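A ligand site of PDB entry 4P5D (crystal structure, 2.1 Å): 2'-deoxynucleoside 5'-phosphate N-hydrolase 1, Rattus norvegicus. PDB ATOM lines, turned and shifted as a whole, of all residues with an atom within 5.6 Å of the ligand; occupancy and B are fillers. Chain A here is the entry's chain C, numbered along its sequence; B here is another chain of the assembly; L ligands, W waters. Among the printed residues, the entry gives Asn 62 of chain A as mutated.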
ATOM      1  N   TYR A   6     -41.179  18.734  22.940  1.00  0.00           N
ATOM      2  CA  TYR A   6     -39.980  18.700  22.101  1.00  0.00           C
ATOM      3  C   TYR A   6     -38.752  18.953  22.986  1.00  0.00           C
ATOM      4  O   TYR A   6     -38.620  20.029  23.568  1.00  0.00           O
ATOM      5  CB  TYR A   6     -40.057  19.755  20.977  1.00  0.00           C
ATOM      6  CG  TYR A   6     -39.007  19.626  19.877  1.00  0.00           C
ATOM      7  CD1 TYR A   6     -37.697  20.048  20.072  1.00  0.00           C
ATOM      8  CD2 TYR A   6     -39.346  19.095  18.627  1.00  0.00           C
ATOM      9  CE1 TYR A   6     -36.748  19.938  19.069  1.00  0.00           C
ATOM     10  CE2 TYR A   6     -38.395  18.972  17.609  1.00  0.00           C
ATOM     11  CZ  TYR A   6     -37.102  19.394  17.843  1.00  0.00           C
ATOM     12  OH  TYR A   6     -36.160  19.281  16.829  1.00  0.00           O
ATOM     13  N   PHE A   7     -37.863  17.972  23.083  1.00  0.00           N
ATOM     14  CA  PHE A   7     -36.637  18.160  23.853  1.00  0.00           C
ATOM     15  C   PHE A   7     -35.434  18.433  22.956  1.00  0.00           C
ATOM     16  O   PHE A   7     -35.171  17.666  22.035  1.00  0.00           O
ATOM     17  CB  PHE A   7     -36.347  16.933  24.742  1.00  0.00           C
ATOM     18  CG  PHE A   7     -35.021  17.032  25.437  1.00  0.00           C
ATOM     19  CD1 PHE A   7     -34.832  17.961  26.446  1.00  0.00           C
ATOM     20  CD2 PHE A   7     -33.965  16.231  25.039  1.00  0.00           C
ATOM     21  CE1 PHE A   7     -33.591  18.083  27.061  1.00  0.00           C
ATOM     22  CE2 PHE A   7     -32.724  16.353  25.654  1.00  0.00           C
ATOM     23  CZ  PHE A   7     -32.540  17.282  26.675  1.00  0.00           C
ATOM     24  N   CYS A   8     -34.699  19.511  23.242  1.00  0.00           N
ATOM     25  CA  CYS A   8     -33.473  19.856  22.523  1.00  0.00           C
ATOM     26  C   CYS A   8     -32.211  19.640  23.359  1.00  0.00           C
ATOM     27  O   CYS A   8     -32.124  20.105  24.490  1.00  0.00           O
ATOM     28  CB  CYS A   8     -33.469  21.329  22.077  1.00  0.00           C
ATOM     29  SG  CYS A   8     -35.003  21.991  21.486  1.00  0.00           S
ATOM     30  N   GLY A   9     -31.226  18.981  22.764  1.00  0.00           N
ATOM     31  CA  GLY A   9     -29.928  18.856  23.400  1.00  0.00           C
ATOM     32  C   GLY A   9     -28.859  18.647  22.346  1.00  0.00           C
ATOM     33  O   GLY A   9     -29.136  18.148  21.259  1.00  0.00           O
ATOM     34  N   SER A  10     -27.622  19.004  22.687  1.00  0.00           N
ATOM     35  CA  SER A  10     -26.527  18.961  21.728  1.00  0.00           C
ATOM     36  C   SER A  10     -26.239  17.548  21.232  1.00  0.00           C
ATOM     37  O   SER A  10     -26.278  16.596  22.004  1.00  0.00           O
ATOM     38  CB  SER A  10     -25.245  19.543  22.340  1.00  0.00           C
ATOM     39  OG  SER A  10     -24.139  19.386  21.470  1.00  0.00           O
ATOM     40  N   ILE A  11     -25.978  17.421  19.932  1.00  0.00           N
ATOM     41  CA  ILE A  11     -25.526  16.148  19.390  1.00  0.00           C
ATOM     42  C   ILE A  11     -24.177  16.350  18.713  1.00  0.00           C
ATOM     43  O   ILE A  11     -23.148  15.992  19.284  1.00  0.00           O
ATOM     44  CB  ILE A  11     -26.560  15.565  18.420  1.00  0.00           C
ATOM     45  CG1 ILE A  11     -27.856  15.277  19.164  1.00  0.00           C
ATOM     46  CG2 ILE A  11     -26.029  14.290  17.765  1.00  0.00           C
ATOM     47  CD1 ILE A  11     -28.982  14.770  18.295  1.00  0.00           C
ATOM     48  N   ARG A  12     -24.143  16.985  17.539  1.00  0.00           N
ATOM     49  CA  ARG A  12     -22.863  17.243  16.888  1.00  0.00           C
ATOM     50  C   ARG A  12     -22.118  18.398  17.560  1.00  0.00           C
ATOM     51  O   ARG A  12     -20.924  18.586  17.339  1.00  0.00           O
ATOM     52  CB  ARG A  12     -23.054  17.481  15.383  1.00  0.00           C
ATOM     53  CG  ARG A  12     -23.223  16.166  14.609  1.00  0.00           C
ATOM     54  CD  ARG A  12     -23.454  16.357  13.103  1.00  0.00           C
ATOM     55  NE  ARG A  12     -23.571  15.065  12.419  1.00  0.00           N
ATOM     56  CZ  ARG A  12     -24.109  14.894  11.213  1.00  0.00           C
ATOM     57  NH1 ARG A  12     -24.593  15.929  10.534  1.00  0.00           N
ATOM     58  NH2 ARG A  12     -24.169  13.675  10.683  1.00  0.00           N
ATOM     59  N   GLY A  13     -22.810  19.158  18.406  1.00  0.00           N
ATOM     60  CA  GLY A  13     -22.135  20.139  19.254  1.00  0.00           C
ATOM     61  C   GLY A  13     -21.344  19.424  20.352  1.00  0.00           C
ATOM     62  O   GLY A  13     -20.552  20.049  21.054  1.00  0.00           O
ATOM     63  N   GLY A  14     -21.524  18.114  20.429  1.00  0.00           N
ATOM     64  CA  GLY A  14     -20.942  17.233  21.432  1.00  0.00           C
ATOM     65  C   GLY A  14     -21.872  16.632  22.476  1.00  0.00           C
ATOM     66  O   GLY A  14     -22.899  17.196  22.832  1.00  0.00           O
ATOM     67  N   THR A  36     -38.846  13.942  20.780  1.00  0.00           N
ATOM     68  CA  THR A  36     -37.406  13.918  20.483  1.00  0.00           C
ATOM     69  C   THR A  36     -36.544  12.939  21.271  1.00  0.00           C
ATOM     70  O   THR A  36     -35.338  13.164  21.392  1.00  0.00           O
ATOM     71  CB  THR A  36     -36.813  15.297  20.613  1.00  0.00           C
ATOM     72  OG1 THR A  36     -37.214  15.868  21.859  1.00  0.00           O
ATOM     73  CG2 THR A  36     -37.347  16.142  19.484  1.00  0.00           C
ATOM     74  N   HIS A  38     -34.911  10.352  21.286  1.00  0.00           N
ATOM     75  CA  HIS A  38     -33.626   9.892  20.761  1.00  0.00           C
ATOM     76  C   HIS A  38     -32.422  10.806  21.062  1.00  0.00           C
ATOM     77  O   HIS A  38     -31.283  10.336  21.058  1.00  0.00           O
ATOM     78  CB  HIS A  38     -33.750   9.733  19.250  1.00  0.00           C
ATOM     79  CG  HIS A  38     -34.292  10.958  18.587  1.00  0.00           C
ATOM     80  ND1 HIS A  38     -35.636  11.192  18.451  1.00  0.00           N
ATOM     81  CD2 HIS A  38     -33.665  12.035  18.064  1.00  0.00           C
ATOM     82  CE1 HIS A  38     -35.820  12.350  17.857  1.00  0.00           C
ATOM     83  NE2 HIS A  38     -34.638  12.892  17.604  1.00  0.00           N
ATOM     84  N   VAL A  39     -32.660  12.098  21.294  1.00  0.00           N
ATOM     85  CA  VAL A  39     -31.587  13.046  21.610  1.00  0.00           C
ATOM     86  C   VAL A  39     -30.833  12.613  22.870  1.00  0.00           C
ATOM     87  O   VAL A  39     -29.639  12.888  23.040  1.00  0.00           O
ATOM     88  CB  VAL A  39     -32.133  14.488  21.810  1.00  0.00           C
ATOM     89  CG1 VAL A  39     -31.007  15.469  22.140  1.00  0.00           C
ATOM     90  CG2 VAL A  39     -32.879  14.954  20.561  1.00  0.00           C
ATOM     91  N   LEU A  44     -26.517   6.894  20.873  1.00  0.00           N
ATOM     92  CA  LEU A  44     -26.311   7.745  19.733  1.00  0.00           C
ATOM     93  C   LEU A  44     -24.972   8.370  20.018  1.00  0.00           C
ATOM     94  O   LEU A  44     -24.790   9.187  20.939  1.00  0.00           O
ATOM     95  CB  LEU A  44     -27.424   8.816  19.622  1.00  0.00           C
ATOM     96  CG  LEU A  44     -27.584   9.755  18.395  1.00  0.00           C
ATOM     97  CD1 LEU A  44     -28.855  10.568  18.515  1.00  0.00           C
ATOM     98  CD2 LEU A  44     -26.432  10.697  18.200  1.00  0.00           C
ATOM     99  N   GLU A  45     -24.015   7.996  19.169  1.00  0.00           N
ATOM    100  CA  GLU A  45     -22.863   8.817  18.974  1.00  0.00           C
ATOM    101  C   GLU A  45     -22.718   8.832  17.474  1.00  0.00           C
ATOM    102  O   GLU A  45     -22.774   7.786  16.818  1.00  0.00           O
ATOM    103  CB  GLU A  45     -21.644   8.239  19.712  1.00  0.00           C
ATOM    104  CG  GLU A  45     -21.896   8.004  21.212  1.00  0.00           C
ATOM    105  CD  GLU A  45     -20.984   6.969  21.852  1.00  0.00           C
ATOM    106  OE1 GLU A  45     -19.865   7.346  22.274  1.00  0.00           O
ATOM    107  OE2 GLU A  45     -21.397   5.789  21.973  1.00  0.00           O
ATOM    108  N   PRO A  46     -22.553  10.046  16.948  1.00  0.00           N
ATOM    109  CA  PRO A  46     -22.295  10.648  15.644  1.00  0.00           C
ATOM    110  C   PRO A  46     -20.830  10.747  15.373  1.00  0.00           C
ATOM    111  O   PRO A  46     -20.000  10.052  15.974  1.00  0.00           O
ATOM    112  CB  PRO A  46     -22.939  12.021  15.765  1.00  0.00           C
ATOM    113  CG  PRO A  46     -22.636  12.387  17.144  1.00  0.00           C
ATOM    114  CD  PRO A  46     -22.753  11.118  17.951  1.00  0.00           C
ATOM    115  N   LEU A  47     -20.559  11.554  14.343  1.00  0.00           N
ATOM    116  CA  LEU A  47     -19.226  11.908  13.852  1.00  0.00           C
ATOM    117  C   LEU A  47     -18.934  10.755  12.886  1.00  0.00           C
ATOM    118  O   LEU A  47     -17.923  10.750  12.169  1.00  0.00           O
ATOM    119  CB  LEU A  47     -18.189  12.093  14.973  1.00  0.00           C
ATOM    120  CG  LEU A  47     -18.639  13.075  16.079  1.00  0.00           C
ATOM    121  CD1 LEU A  47     -17.434  13.509  16.911  1.00  0.00           C
ATOM    122  CD2 LEU A  47     -19.451  14.299  15.573  1.00  0.00           C
ATOM    123  N   GLU A  49     -21.415  10.533  10.487  1.00  0.00           N
ATOM    124  CA  GLU A  49     -22.190  10.995   9.280  1.00  0.00           C
ATOM    125  C   GLU A  49     -23.435  10.212   8.780  1.00  0.00           C
ATOM    126  O   GLU A  49     -23.880  10.457   7.653  1.00  0.00           O
ATOM    127  CB  GLU A  49     -21.320  11.190   8.056  1.00  0.00           C
ATOM    128  CG  GLU A  49     -21.153  12.676   7.783  1.00  0.00           C
ATOM    129  CD  GLU A  49     -19.695  13.049   7.763  1.00  0.00           C
ATOM    130  OE1 GLU A  49     -19.302  13.961   6.983  1.00  0.00           O
ATOM    131  OE2 GLU A  49     -18.963  12.407   8.539  1.00  0.00           O
ATOM    132  N   GLU A  50     -23.910   9.213   9.511  1.00  0.00           N
ATOM    133  CA  GLU A  50     -25.071   8.353   9.099  1.00  0.00           C
ATOM    134  C   GLU A  50     -26.459   9.039   9.216  1.00  0.00           C
ATOM    135  O   GLU A  50     -26.575  10.279   9.155  1.00  0.00           O
ATOM    136  CB  GLU A  50     -25.084   7.044   9.894  1.00  0.00           C
ATOM    137  CG  GLU A  50     -24.986   5.747   9.015  1.00  0.00           C
ATOM    138  CD  GLU A  50     -25.892   4.603   9.485  1.00  0.00           C
ATOM    139  OE1 GLU A  50     -27.088   4.862   9.685  1.00  0.00           O
ATOM    140  OE2 GLU A  50     -25.423   3.446   9.630  1.00  0.00           O
ATOM    141  N   ALA A  51     -27.483   8.188   9.380  1.00  0.00           N
ATOM    142  CA  ALA A  51     -28.956   8.375   9.291  1.00  0.00           C
ATOM    143  C   ALA A  51     -29.612   8.035   7.958  1.00  0.00           C
ATOM    144  O   ALA A  51     -30.861   8.006   7.875  1.00  0.00           O
ATOM    145  CB  ALA A  51     -29.329   9.843   9.653  1.00  0.00           C
ATOM    146  N   ILE A  58     -33.721  14.405   8.540  1.00  0.00           N
ATOM    147  CA  ILE A  58     -33.616  14.805   9.930  1.00  0.00           C
ATOM    148  C   ILE A  58     -34.244  16.173  10.149  1.00  0.00           C
ATOM    149  O   ILE A  58     -35.078  16.350  11.047  1.00  0.00           O
ATOM    150  CB  ILE A  58     -32.140  14.864  10.389  1.00  0.00           C
ATOM    151  CG1 ILE A  58     -31.513  13.468  10.314  1.00  0.00           C
ATOM    152  CG2 ILE A  58     -32.042  15.427  11.808  1.00  0.00           C
ATOM    153  CD1 ILE A  58     -32.239  12.429  11.117  1.00  0.00           C
ATOM    154  N   ASN A  62     -37.792  16.742  12.232  1.00  0.00           N
ATOM    155  CA  ASN A  62     -37.756  17.549  13.445  1.00  0.00           C
ATOM    156  C   ASN A  62     -38.685  18.760  13.410  1.00  0.00           C
ATOM    157  O   ASN A  62     -39.342  19.076  14.396  1.00  0.00           O
ATOM    158  CB  ASN A  62     -36.332  17.987  13.740  1.00  0.00           C
ATOM    159  CG  ASN A  62     -35.575  16.915  14.415  1.00  0.00           C
ATOM    160  OD1 ASN A  62     -36.169  16.001  14.983  1.00  0.00           O
ATOM    161  ND2 ASN A  62     -34.261  17.005  14.396  1.00  0.00           N
ATOM    162  N   PRO A  79     -22.808  24.322  23.945  1.00  0.00           N
ATOM    163  CA  PRO A  79     -23.118  25.110  22.747  1.00  0.00           C
ATOM    164  C   PRO A  79     -23.373  24.226  21.520  1.00  0.00           C
ATOM    165  O   PRO A  79     -22.607  23.308  21.246  1.00  0.00           O
ATOM    166  CB  PRO A  79     -21.861  25.975  22.533  1.00  0.00           C
ATOM    167  CG  PRO A  79     -21.245  26.088  23.916  1.00  0.00           C
ATOM    168  CD  PRO A  79     -21.535  24.734  24.560  1.00  0.00           C
ATOM    169  N   SER A  80     -24.483  24.484  20.831  1.00  0.00           N
ATOM    170  CA  SER A  80     -24.910  23.689  19.689  1.00  0.00           C
ATOM    171  C   SER A  80     -25.639  24.560  18.671  1.00  0.00           C
ATOM    172  O   SER A  80     -26.568  25.288  19.022  1.00  0.00           O
ATOM    173  CB  SER A  80     -25.821  22.546  20.171  1.00  0.00           C
ATOM    174  OG  SER A  80     -26.588  21.987  19.105  1.00  0.00           O
ATOM    175  N   LEU A  81     -25.286  24.430  17.394  1.00  0.00           N
ATOM    176  CA  LEU A  81     -26.013  25.117  16.337  1.00  0.00           C
ATOM    177  C   LEU A  81     -27.455  24.611  16.248  1.00  0.00           C
ATOM    178  O   LEU A  81     -28.409  25.386  16.116  1.00  0.00           O
ATOM    179  CB  LEU A  81     -25.332  24.927  14.987  1.00  0.00           C
ATOM    180  CG  LEU A  81     -23.947  25.528  14.801  1.00  0.00           C
ATOM    181  CD1 LEU A  81     -23.351  24.998  13.506  1.00  0.00           C
ATOM    182  CD2 LEU A  81     -24.035  27.069  14.784  1.00  0.00           C
ATOM    183  N   GLY A  82     -27.593  23.291  16.297  1.00  0.00           N
ATOM    184  CA  GLY A  82     -28.908  22.672  16.182  1.00  0.00           C
ATOM    185  C   GLY A  82     -29.872  23.128  17.266  1.00  0.00           C
ATOM    186  O   GLY A  82     -31.014  23.473  16.993  1.00  0.00           O
ATOM    187  N   VAL A  83     -29.399  23.105  18.506  1.00  0.00           N
ATOM    188  CA  VAL A  83     -30.239  23.554  19.617  1.00  0.00           C
ATOM    189  C   VAL A  83     -30.637  25.025  19.427  1.00  0.00           C
ATOM    190  O   VAL A  83     -31.821  25.371  19.564  1.00  0.00           O
ATOM    191  CB  VAL A  83     -29.521  23.354  20.963  1.00  0.00           C
ATOM    192  CG1 VAL A  83     -30.317  23.989  22.087  1.00  0.00           C
ATOM    193  CG2 VAL A  83     -29.316  21.882  21.235  1.00  0.00           C
ATOM    194  N   GLU A  86     -33.269  25.249  16.611  1.00  0.00           N
ATOM    195  CA  GLU A  86     -34.575  24.783  17.097  1.00  0.00           C
ATOM    196  C   GLU A  86     -35.250  25.843  17.959  1.00  0.00           C
ATOM    197  O   GLU A  86     -36.440  26.121  17.796  1.00  0.00           O
ATOM    198  CB  GLU A  86     -34.426  23.467  17.882  1.00  0.00           C
ATOM    199  CG  GLU A  86     -34.081  22.263  16.991  1.00  0.00           C
ATOM    200  CD  GLU A  86     -33.626  21.014  17.763  1.00  0.00           C
ATOM    201  OE1 GLU A  86     -33.951  19.901  17.309  1.00  0.00           O
ATOM    202  OE2 GLU A  86     -32.938  21.137  18.809  1.00  0.00           O
ATOM    203  N   SER B 110     -23.700  20.443  11.909  1.00  0.00           N
ATOM    204  CA  SER B 110     -25.018  20.116  12.445  1.00  0.00           C
ATOM    205  C   SER B 110     -26.009  19.683  11.372  1.00  0.00           C
ATOM    206  O   SER B 110     -26.146  20.354  10.343  1.00  0.00           O
ATOM    207  CB  SER B 110     -25.603  21.324  13.170  1.00  0.00           C
ATOM    208  OG  SER B 110     -26.926  21.061  13.582  1.00  0.00           O
ATOM    209  N   ALA B 111     -26.716  18.588  11.625  1.00  0.00           N
ATOM    210  CA  ALA B 111     -27.731  18.105  10.702  1.00  0.00           C
ATOM    211  C   ALA B 111     -28.838  19.133  10.509  1.00  0.00           C
ATOM    212  O   ALA B 111     -29.459  19.184   9.462  1.00  0.00           O
ATOM    213  CB  ALA B 111     -28.332  16.772  11.173  1.00  0.00           C
ATOM    214  N   MET B 112     -29.107  19.933  11.536  1.00  0.00           N
ATOM    215  CA  MET B 112     -30.193  20.897  11.427  1.00  0.00           C
ATOM    216  C   MET B 112     -29.807  22.080  10.555  1.00  0.00           C
ATOM    217  O   MET B 112     -30.664  22.787  10.034  1.00  0.00           O
ATOM    218  CB  MET B 112     -30.639  21.380  12.814  1.00  0.00           C
ATOM    219  CG  MET B 112     -31.257  20.291  13.669  1.00  0.00           C
ATOM    220  SD  MET B 112     -32.759  19.626  12.928  1.00  0.00           S
ATOM    221  CE  MET B 112     -33.924  20.978  13.073  1.00  0.00           C
HETATM  222  C1  LIG L   1     -29.002  11.575  13.848  1.00  0.00           C
HETATM  223  C2  LIG L   1     -27.915  10.809  13.408  1.00  0.00           C
HETATM  224  C3  LIG L   1     -28.090   9.440  13.136  1.00  0.00           C
HETATM  225  C4  LIG L   1     -27.014   8.667  12.715  1.00  0.00           C
HETATM  226  C5  LIG L   1     -25.762   9.254  12.559  1.00  0.00           C
HETATM  227  C6  LIG L   1     -25.591  10.616  12.837  1.00  0.00           C
HETATM  228  C7  LIG L   1     -26.668  11.390  13.258  1.00  0.00           C
HETATM  229  C8  LIG L   1     -26.488  12.741  13.532  1.00  0.00           C
HETATM  230  C9  LIG L   1     -27.556  13.511  13.957  1.00  0.00           C
HETATM  231  C10 LIG L   1     -28.837  12.930  14.078  1.00  0.00           C
HETATM  232  C11 LIG L   1     -30.014  13.730  14.603  1.00  0.00           C
HETATM  233  N1  LIG L   1     -31.208  13.116  14.760  1.00  0.00           N
HETATM  234  C12 LIG L   1     -32.269  13.735  15.278  1.00  0.00           C
HETATM  235  N2  LIG L   1     -32.218  15.029  15.675  1.00  0.00           N
HETATM  236  C13 LIG L   1     -31.054  15.730  15.560  1.00  0.00           C
HETATM  237  C14 LIG L   1     -29.902  15.090  15.026  1.00  0.00           C
HETATM  238  N3  LIG L   1     -28.903  16.024  15.029  1.00  0.00           N
HETATM  239  C15 LIG L   1     -29.394  17.170  15.547  1.00  0.00           C
HETATM  240  N4  LIG L   1     -30.675  17.011  15.870  1.00  0.00           N
HETATM  241  C16 LIG L   1     -31.507  17.943  16.461  1.00  0.00           C
HETATM  242  O1  LIG L   1     -30.589  19.238  16.754  1.00  0.00           O
HETATM  243  C17 LIG L   1     -31.852  17.465  17.676  1.00  0.00           C
HETATM  244  O2  LIG L   1     -33.306  17.569  17.969  1.00  0.00           O
HETATM  245  C18 LIG L   1     -31.064  18.230  18.775  1.00  0.00           C
HETATM  246  O3  LIG L   1     -31.848  18.874  19.651  1.00  0.00           O
HETATM  247  C19 LIG L   1     -30.206  19.272  18.018  1.00  0.00           C
HETATM  248  C20 LIG L   1     -28.723  18.954  18.156  1.00  0.00           C
HETATM  249  O4  LIG L   1     -28.021  19.887  17.312  1.00  0.00           O
HETATM  250  P1  LIG L   1     -26.469  19.682  17.020  1.00  0.00           P
HETATM  251  O5  LIG L   1     -26.256  18.377  16.357  1.00  0.00           O
HETATM  252  O6  LIG L   1     -26.032  20.846  16.115  1.00  0.00           O
HETATM  253  O7  LIG L   1     -25.703  19.729  18.312  1.00  0.00           O
HETATM  254  O   HOH W   1     -26.390  17.117  14.055  1.00  0.00           O
HETATM  255  O   HOH W   2     -32.804  10.473  14.745  1.00  0.00           O
HETATM  256  O   HOH W   3     -23.687  22.039  16.579  1.00  0.00           O
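Tyr 6 touches the ligand (OH to O2, 3.5 Å).
Cys 8 touches the ligand (CA to O3, 3.4 Å).
Ser 10 touches the ligand (OG to O7, 3.5 Å).
His 38 touches the ligand.
CG2 of Val 39 touches O2 of the ligand, 3.7 Å away.
C of Glu 50 touches C5 of the ligand, at 3.4 Å.
Ala 51 touches the ligand.
Ile 58 touches the ligand (CG2 to N1, 3.8 Å).
N of Leu 81 touches O6 of the ligand, at 3.9 Å.
N of Val 83 touches O4 of the ligand, at 3.7 Å.
Ala 111 of chain B touches the ligand (CB to N3, 3.97 Å).
Met 112 of chain B touches the ligand.
Within 4 Å of the ligand: Tyr 6, Cys 8, Gly 9, Ser 10, Ile 11, Arg 12, Gly 13, His 38, Val 39, Glu 50, Ala 51, Ile 58, Asn 62, Ser 80, Leu 81, Gly 82, Val 83, Glu 86, Ser 110 of chain B, Ala 111 of chain B and Met 112 of chain B.
The nearest printed residue that does not touch the ligand is Pro 46 (4.2 Å).
OE1 of Glu 86 sits at hydrogen-bond distance from O2 of the ligand (2.5 Å).
An oxygen (O7) of the ligand sits at hydrogen-bond distance from the side-chain hydroxyl of Ser 80, 2.6 Å away.
The side-chain hydroxyl of Ser 110 of chain B sits at hydrogen-bond distance from an oxygen (O6) of the ligand (2.7 Å).
O5 of the ligand is in hydrogen-bond range of N of Arg 12 (2.8 Å).
The backbone NH (N) of Ile 11 is in hydrogen-bond range of an oxygen (O7) of the ligand, at 2.8 Å.
An oxygen (O6) of the ligand lies within hydrogen-bond range of the backbone NH (N) of Gly 82 (2.9 Å).
N of Gly 13 sits at hydrogen-bond distance from O7 of the ligand, 3.0 Å away.
A nitrogen (N2) of the ligand sits at hydrogen-bond distance from the side-chain amide nitrogen (ND2) of Asn 62 (3.1 Å).
N of Gly 9 lies within hydrogen-bond range of O3 of the ligand.
O of Gly 9 sits close to O3 of the ligand.
The side-chain carboxylate (OE2) of Glu 86 lies close to the side-chain sulfur (SG) of Cys 8 (3.5 Å).
N of Gly 82 is in hydrogen-bond range of OG of Ser 80 (3.3 Å).
The side-chain hydroxyl (OG) of Ser 80 sits at hydrogen-bond distance from the backbone NH (N) of Val 83.
OG of Ser 110 of chain B lies close to N of Met 112 of chain B, 3.2 Å away.
The side-chain hydroxyl (OG) of Ser 10 sits close to the backbone NH (N) of Gly 13.
The side-chain amide nitrogen (ND2) of Asn 62 sits at hydrogen-bond distance from the side-chain sulfur (SD) of Met 112 of chain B (3.4 Å).
O of Gly 14 lies within hydrogen-bond range of OG of Ser 10, 2.9 Å away.
Water W1 lies within hydrogen-bond range of an oxygen (O5) of the ligand (2.6 Å) and the backbone NH (N) of Ala 111 of chain B (2.9 Å).
Water W3 bridges an oxygen (O6) of the ligand (2.7 Å) and the backbone NH (N) of Leu 81 (3.0 Å).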
